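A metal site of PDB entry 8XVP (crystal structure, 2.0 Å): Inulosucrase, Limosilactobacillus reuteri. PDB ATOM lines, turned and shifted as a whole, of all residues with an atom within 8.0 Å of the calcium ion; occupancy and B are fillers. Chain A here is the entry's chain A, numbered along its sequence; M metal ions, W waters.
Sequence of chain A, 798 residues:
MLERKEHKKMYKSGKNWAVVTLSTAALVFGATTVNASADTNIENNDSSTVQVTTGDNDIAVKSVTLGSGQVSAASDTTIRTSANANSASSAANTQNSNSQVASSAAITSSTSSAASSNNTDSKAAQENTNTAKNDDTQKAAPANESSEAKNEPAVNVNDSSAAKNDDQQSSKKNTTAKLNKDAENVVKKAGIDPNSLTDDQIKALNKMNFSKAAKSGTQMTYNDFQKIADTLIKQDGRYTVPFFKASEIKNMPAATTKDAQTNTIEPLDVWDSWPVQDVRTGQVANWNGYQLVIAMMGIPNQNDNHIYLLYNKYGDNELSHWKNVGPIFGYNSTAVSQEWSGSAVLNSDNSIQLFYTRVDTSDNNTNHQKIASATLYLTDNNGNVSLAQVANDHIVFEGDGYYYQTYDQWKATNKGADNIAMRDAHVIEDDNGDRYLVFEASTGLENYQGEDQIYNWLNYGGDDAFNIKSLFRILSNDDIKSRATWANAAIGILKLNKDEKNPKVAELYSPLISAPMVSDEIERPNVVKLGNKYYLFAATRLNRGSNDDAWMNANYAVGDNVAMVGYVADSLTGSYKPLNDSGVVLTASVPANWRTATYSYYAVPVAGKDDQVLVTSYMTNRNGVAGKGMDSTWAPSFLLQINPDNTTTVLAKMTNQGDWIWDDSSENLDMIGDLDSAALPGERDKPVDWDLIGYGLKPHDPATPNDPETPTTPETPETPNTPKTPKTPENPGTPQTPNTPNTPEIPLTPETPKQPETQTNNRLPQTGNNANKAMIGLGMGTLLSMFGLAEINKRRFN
The calcium ion is bound by O of Ile 661.
Water W1 binds the calcium ion (2.3 Å).
OD1 of Asn 317 is bound to the calcium ion (2.3 Å).
The side-chain hydroxyl (OG) of Ser 666 is bound to the calcium ion, at 2.3 Å.
The calcium ion is bound by OD1 of Asp 659, 2.3 Å away.
Water W2 binds the calcium ion, at 2.3 Å.
OD2 of Asp 659 binds the calcium ion (2.4 Å).
The calcium ion has seven donor atoms within binding distance.
Four residues have an atom within 4 Å of the calcium ion: Asn 317, Asp 659, Ile 661 and Ser 666.
Water W2 lies within hydrogen-bond range of the side-chain carboxylate (OD2) of Asp 663 (2.7 Å) and the backbone carbonyl oxygen (O) of Gly 315 (2.8 Å).
The side-chain amide oxygen (OD1) of Asn 317 lies close to the backbone carbonyl oxygen (O) of Gly 315.
The side-chain amide nitrogen of Asn 317 is in hydrogen-bond range of the side-chain hydroxyl of Ser 665 (3.3 Å).
The side-chain amide nitrogen of Asn 656 lies within hydrogen-bond range of the backbone carbonyl oxygen of Asn 317 (3.0 Å).
The backbone NH of Ser 666 sits at hydrogen-bond distance from the side-chain carboxylate of Asp 663 (3.3 Å).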
ATOM      1  N   GLN A 291     -34.254 -16.438   5.070  1.00  0.00           N
ATOM      2  CA  GLN A 291     -34.429 -17.728   4.414  1.00  0.00           C
ATOM      3  C   GLN A 291     -35.289 -18.612   5.319  1.00  0.00           C
ATOM      4  O   GLN A 291     -35.199 -18.543   6.567  1.00  0.00           O
ATOM      5  CB  GLN A 291     -33.095 -18.428   4.142  1.00  0.00           C
ATOM      6  CG  GLN A 291     -32.190 -18.627   5.350  1.00  0.00           C
ATOM      7  CD  GLN A 291     -30.864 -19.258   4.975  1.00  0.00           C
ATOM      8  OE1 GLN A 291     -30.815 -20.146   4.149  1.00  0.00           O
ATOM      9  NE2 GLN A 291     -29.784 -18.785   5.569  1.00  0.00           N
ATOM     10  N   LYS A 313     -31.438 -15.648   8.967  1.00  0.00           N
ATOM     11  CA  LYS A 313     -31.218 -14.512   8.069  1.00  0.00           C
ATOM     12  C   LYS A 313     -30.789 -15.044   6.715  1.00  0.00           C
ATOM     13  O   LYS A 313     -29.977 -15.973   6.628  1.00  0.00           O
ATOM     14  CB  LYS A 313     -30.135 -13.586   8.645  1.00  0.00           C
ATOM     15  CG  LYS A 313     -30.519 -12.899   9.963  1.00  0.00           C
ATOM     16  CD  LYS A 313     -31.208 -11.569   9.706  1.00  0.00           C
ATOM     17  CE  LYS A 313     -32.001 -11.101  10.920  1.00  0.00           C
ATOM     18  NZ  LYS A 313     -32.869  -9.962  10.519  1.00  0.00           N
ATOM     19  N   TYR A 314     -31.317 -14.462   5.649  1.00  0.00           N
ATOM     20  CA  TYR A 314     -30.977 -14.890   4.319  1.00  0.00           C
ATOM     21  C   TYR A 314     -29.465 -14.784   4.115  1.00  0.00           C
ATOM     22  O   TYR A 314     -28.881 -13.759   4.413  1.00  0.00           O
ATOM     23  CB  TYR A 314     -31.690 -14.037   3.255  1.00  0.00           C
ATOM     24  CG  TYR A 314     -31.492 -14.574   1.860  1.00  0.00           C
ATOM     25  CD1 TYR A 314     -30.343 -14.265   1.112  1.00  0.00           C
ATOM     26  CD2 TYR A 314     -32.420 -15.441   1.312  1.00  0.00           C
ATOM     27  CE1 TYR A 314     -30.156 -14.806  -0.156  1.00  0.00           C
ATOM     28  CE2 TYR A 314     -32.232 -15.963   0.028  1.00  0.00           C
ATOM     29  CZ  TYR A 314     -31.116 -15.638  -0.692  1.00  0.00           C
ATOM     30  OH  TYR A 314     -30.997 -16.188  -1.934  1.00  0.00           O
ATOM     31  N   GLY A 315     -28.825 -15.846   3.637  1.00  0.00           N
ATOM     32  CA  GLY A 315     -27.385 -15.830   3.379  1.00  0.00           C
ATOM     33  C   GLY A 315     -26.518 -16.227   4.573  1.00  0.00           C
ATOM     34  O   GLY A 315     -25.321 -16.469   4.424  1.00  0.00           O
ATOM     35  N   ASP A 316     -27.119 -16.292   5.757  1.00  0.00           N
ATOM     36  CA  ASP A 316     -26.395 -16.734   6.961  1.00  0.00           C
ATOM     37  C   ASP A 316     -25.963 -18.199   6.830  1.00  0.00           C
ATOM     38  O   ASP A 316     -26.757 -19.041   6.373  1.00  0.00           O
ATOM     39  CB  ASP A 316     -27.277 -16.542   8.196  1.00  0.00           C
ATOM     40  CG  ASP A 316     -26.587 -16.978   9.473  1.00  0.00           C
ATOM     41  OD1 ASP A 316     -26.309 -18.187   9.649  1.00  0.00           O
ATOM     42  OD2 ASP A 316     -26.336 -16.106  10.321  1.00  0.00           O
ATOM     43  N   ASN A 317     -24.712 -18.481   7.222  1.00  0.00           N
ATOM     44  CA  ASN A 317     -24.084 -19.764   6.976  1.00  0.00           C
ATOM     45  C   ASN A 317     -23.888 -20.656   8.221  1.00  0.00           C
ATOM     46  O   ASN A 317     -23.205 -21.669   8.144  1.00  0.00           O
ATOM     47  CB  ASN A 317     -22.730 -19.534   6.325  1.00  0.00           C
ATOM     48  CG  ASN A 317     -22.861 -18.968   4.933  1.00  0.00           C
ATOM     49  OD1 ASN A 317     -23.761 -19.360   4.161  1.00  0.00           O
ATOM     50  ND2 ASN A 317     -21.970 -18.050   4.591  1.00  0.00           N
ATOM     51  N   GLU A 318     -24.489 -20.282   9.338  1.00  0.00           N
ATOM     52  CA  GLU A 318     -24.246 -21.010  10.585  1.00  0.00           C
ATOM     53  C   GLU A 318     -25.412 -21.894  10.971  1.00  0.00           C
ATOM     54  O   GLU A 318     -26.513 -21.409  11.129  1.00  0.00           O
ATOM     55  CB  GLU A 318     -23.928 -20.005  11.694  1.00  0.00           C
ATOM     56  CG  GLU A 318     -22.935 -18.963  11.123  1.00  0.00           C
ATOM     57  CD  GLU A 318     -21.842 -18.558  12.060  1.00  0.00           C
ATOM     58  OE1 GLU A 318     -21.201 -19.472  12.644  1.00  0.00           O
ATOM     59  OE2 GLU A 318     -21.624 -17.339  12.192  1.00  0.00           O
ATOM     60  N   LEU A 614     -26.625 -26.640  -5.763  1.00  0.00           N
ATOM     61  CA  LEU A 614     -26.150 -26.977  -4.455  1.00  0.00           C
ATOM     62  C   LEU A 614     -26.956 -28.170  -3.941  1.00  0.00           C
ATOM     63  O   LEU A 614     -28.203 -28.070  -3.831  1.00  0.00           O
ATOM     64  CB  LEU A 614     -26.375 -25.793  -3.509  1.00  0.00           C
ATOM     65  CG  LEU A 614     -25.907 -25.997  -2.072  1.00  0.00           C
ATOM     66  CD1 LEU A 614     -24.400 -26.136  -1.985  1.00  0.00           C
ATOM     67  CD2 LEU A 614     -26.370 -24.838  -1.266  1.00  0.00           C
ATOM     68  N   THR A 655     -20.022 -26.621   1.883  1.00  0.00           N
ATOM     69  CA  THR A 655     -20.433 -25.537   2.782  1.00  0.00           C
ATOM     70  C   THR A 655     -20.407 -26.036   4.211  1.00  0.00           C
ATOM     71  O   THR A 655     -20.031 -27.180   4.479  1.00  0.00           O
ATOM     72  CB  THR A 655     -21.886 -25.132   2.489  1.00  0.00           C
ATOM     73  OG1 THR A 655     -22.796 -26.133   3.002  1.00  0.00           O
ATOM     74  CG2 THR A 655     -22.105 -24.950   1.005  1.00  0.00           C
ATOM     75  N   ASN A 656     -20.850 -25.201   5.144  1.00  0.00           N
ATOM     76  CA  ASN A 656     -21.147 -25.680   6.477  1.00  0.00           C
ATOM     77  C   ASN A 656     -22.406 -26.520   6.437  1.00  0.00           C
ATOM     78  O   ASN A 656     -23.105 -26.509   5.412  1.00  0.00           O
ATOM     79  CB  ASN A 656     -21.362 -24.524   7.430  1.00  0.00           C
ATOM     80  CG  ASN A 656     -20.105 -23.684   7.595  1.00  0.00           C
ATOM     81  OD1 ASN A 656     -18.992 -24.190   7.464  1.00  0.00           O
ATOM     82  ND2 ASN A 656     -20.287 -22.387   7.837  1.00  0.00           N
ATOM     83  N   GLY A 658     -26.102 -27.489   6.755  1.00  0.00           N
ATOM     84  CA  GLY A 658     -27.364 -26.803   6.631  1.00  0.00           C
ATOM     85  C   GLY A 658     -27.334 -25.510   5.852  1.00  0.00           C
ATOM     86  O   GLY A 658     -28.159 -24.655   6.097  1.00  0.00           O
ATOM     87  N   ASP A 659     -26.391 -25.356   4.929  1.00  0.00           N
ATOM     88  CA  ASP A 659     -26.387 -24.178   4.061  1.00  0.00           C
ATOM     89  C   ASP A 659     -27.202 -24.393   2.794  1.00  0.00           C
ATOM     90  O   ASP A 659     -26.905 -25.272   1.996  1.00  0.00           O
ATOM     91  CB  ASP A 659     -24.949 -23.827   3.683  1.00  0.00           C
ATOM     92  CG  ASP A 659     -24.833 -22.445   2.979  1.00  0.00           C
ATOM     93  OD1 ASP A 659     -25.892 -21.864   2.657  1.00  0.00           O
ATOM     94  OD2 ASP A 659     -23.688 -21.984   2.708  1.00  0.00           O
ATOM     95  N   TRP A 660     -28.241 -23.573   2.620  1.00  0.00           N
ATOM     96  CA  TRP A 660     -29.157 -23.692   1.487  1.00  0.00           C
ATOM     97  C   TRP A 660     -28.861 -22.750   0.340  1.00  0.00           C
ATOM     98  O   TRP A 660     -29.473 -22.849  -0.730  1.00  0.00           O
ATOM     99  CB  TRP A 660     -30.589 -23.490   1.962  1.00  0.00           C
ATOM    100  CG  TRP A 660     -30.980 -24.505   2.946  1.00  0.00           C
ATOM    101  CD1 TRP A 660     -30.765 -24.469   4.293  1.00  0.00           C
ATOM    102  CD2 TRP A 660     -31.672 -25.719   2.688  1.00  0.00           C
ATOM    103  NE1 TRP A 660     -31.266 -25.583   4.883  1.00  0.00           N
ATOM    104  CE2 TRP A 660     -31.831 -26.380   3.923  1.00  0.00           C
ATOM    105  CE3 TRP A 660     -32.180 -26.314   1.530  1.00  0.00           C
ATOM    106  CZ2 TRP A 660     -32.469 -27.615   4.034  1.00  0.00           C
ATOM    107  CZ3 TRP A 660     -32.822 -27.539   1.638  1.00  0.00           C
ATOM    108  CH2 TRP A 660     -32.934 -28.178   2.885  1.00  0.00           C
ATOM    109  N   ILE A 661     -27.909 -21.854   0.555  1.00  0.00           N
ATOM    110  CA  ILE A 661     -27.638 -20.787  -0.387  1.00  0.00           C
ATOM    111  C   ILE A 661     -26.185 -20.746  -0.778  1.00  0.00           C
ATOM    112  O   ILE A 661     -25.358 -20.326   0.000  1.00  0.00           O
ATOM    113  CB  ILE A 661     -28.044 -19.410   0.196  1.00  0.00           C
ATOM    114  CG1 ILE A 661     -29.537 -19.388   0.549  1.00  0.00           C
ATOM    115  CG2 ILE A 661     -27.719 -18.279  -0.799  1.00  0.00           C
ATOM    116  CD1 ILE A 661     -29.898 -18.376   1.603  1.00  0.00           C
ATOM    117  N   TRP A 662     -25.845 -21.152  -1.989  1.00  0.00           N
ATOM    118  CA  TRP A 662     -24.433 -21.076  -2.357  1.00  0.00           C
ATOM    119  C   TRP A 662     -24.096 -19.648  -2.772  1.00  0.00           C
ATOM    120  O   TRP A 662     -24.818 -19.031  -3.547  1.00  0.00           O
ATOM    121  CB  TRP A 662     -24.039 -22.023  -3.463  1.00  0.00           C
ATOM    122  CG  TRP A 662     -22.596 -21.853  -3.818  1.00  0.00           C
ATOM    123  CD1 TRP A 662     -22.101 -21.066  -4.813  1.00  0.00           C
ATOM    124  CD2 TRP A 662     -21.472 -22.440  -3.165  1.00  0.00           C
ATOM    125  NE1 TRP A 662     -20.752 -21.146  -4.841  1.00  0.00           N
ATOM    126  CE2 TRP A 662     -20.331 -21.990  -3.839  1.00  0.00           C
ATOM    127  CE3 TRP A 662     -21.328 -23.324  -2.097  1.00  0.00           C
ATOM    128  CZ2 TRP A 662     -19.042 -22.389  -3.478  1.00  0.00           C
ATOM    129  CZ3 TRP A 662     -20.039 -23.725  -1.745  1.00  0.00           C
ATOM    130  CH2 TRP A 662     -18.919 -23.255  -2.435  1.00  0.00           C
ATOM    131  N   ASP A 663     -22.996 -19.142  -2.251  1.00  0.00           N
ATOM    132  CA  ASP A 663     -22.359 -17.937  -2.791  1.00  0.00           C
ATOM    133  C   ASP A 663     -20.873 -17.965  -2.433  1.00  0.00           C
ATOM    134  O   ASP A 663     -20.379 -18.958  -1.871  1.00  0.00           O
ATOM    135  CB  ASP A 663     -23.075 -16.682  -2.273  1.00  0.00           C
ATOM    136  CG  ASP A 663     -23.155 -16.658  -0.774  1.00  0.00           C
ATOM    137  OD1 ASP A 663     -22.205 -17.130  -0.135  1.00  0.00           O
ATOM    138  OD2 ASP A 663     -24.170 -16.191  -0.239  1.00  0.00           O
ATOM    139  N   ASP A 664     -20.147 -16.894  -2.781  1.00  0.00           N
ATOM    140  CA  ASP A 664     -18.725 -16.781  -2.503  1.00  0.00           C
ATOM    141  C   ASP A 664     -18.352 -16.763  -1.013  1.00  0.00           C
ATOM    142  O   ASP A 664     -17.212 -17.028  -0.673  1.00  0.00           O
ATOM    143  CB  ASP A 664     -18.141 -15.545  -3.176  1.00  0.00           C
ATOM    144  CG  ASP A 664     -18.193 -15.628  -4.693  1.00  0.00           C
ATOM    145  OD1 ASP A 664     -17.871 -16.708  -5.245  1.00  0.00           O
ATOM    146  OD2 ASP A 664     -18.569 -14.608  -5.331  1.00  0.00           O
ATOM    147  N   SER A 665     -19.312 -16.482  -0.144  1.00  0.00           N
ATOM    148  CA  SER A 665     -19.086 -16.493   1.299  1.00  0.00           C
ATOM    149  C   SER A 665     -19.188 -17.896   1.905  1.00  0.00           C
ATOM    150  O   SER A 665     -18.834 -18.110   3.068  1.00  0.00           O
ATOM    151  CB  SER A 665     -20.135 -15.608   1.984  1.00  0.00           C
ATOM    152  OG  SER A 665     -21.448 -16.214   1.940  1.00  0.00           O
ATOM    153  N   SER A 666     -19.724 -18.844   1.123  1.00  0.00           N
ATOM    154  CA  SER A 666     -20.265 -20.092   1.693  1.00  0.00           C
ATOM    155  C   SER A 666     -19.290 -21.262   1.742  1.00  0.00           C
ATOM    156  O   SER A 666     -19.502 -22.208   2.511  1.00  0.00           O
ATOM    157  CB  SER A 666     -21.527 -20.514   0.945  1.00  0.00           C
ATOM    158  OG  SER A 666     -22.598 -19.642   1.249  1.00  0.00           O
ATOM    159  N   GLU A 667     -18.248 -21.218   0.921  1.00  0.00           N
ATOM    160  CA  GLU A 667     -17.294 -22.327   0.901  1.00  0.00           C
ATOM    161  C   GLU A 667     -16.660 -22.514   2.274  1.00  0.00           C
ATOM    162  O   GLU A 667     -16.252 -21.567   2.916  1.00  0.00           O
ATOM    163  CB  GLU A 667     -16.216 -22.134  -0.164  1.00  0.00           C
ATOM    164  CG  GLU A 667     -15.208 -23.279  -0.269  1.00  0.00           C
ATOM    165  CD  GLU A 667     -14.461 -23.311  -1.577  1.00  0.00           C
ATOM    166  OE1 GLU A 667     -14.580 -22.353  -2.376  1.00  0.00           O
ATOM    167  OE2 GLU A 667     -13.756 -24.304  -1.818  1.00  0.00           O
HETATM  168 CA    CA M   1     -24.704 -19.925   2.137  1.00  0.00          CA
HETATM  169  O   HOH W   1     -26.521 -19.486   3.478  1.00  0.00           O
HETATM  170  O   HOH W   2     -24.712 -17.595   1.983  1.00  0.00           O
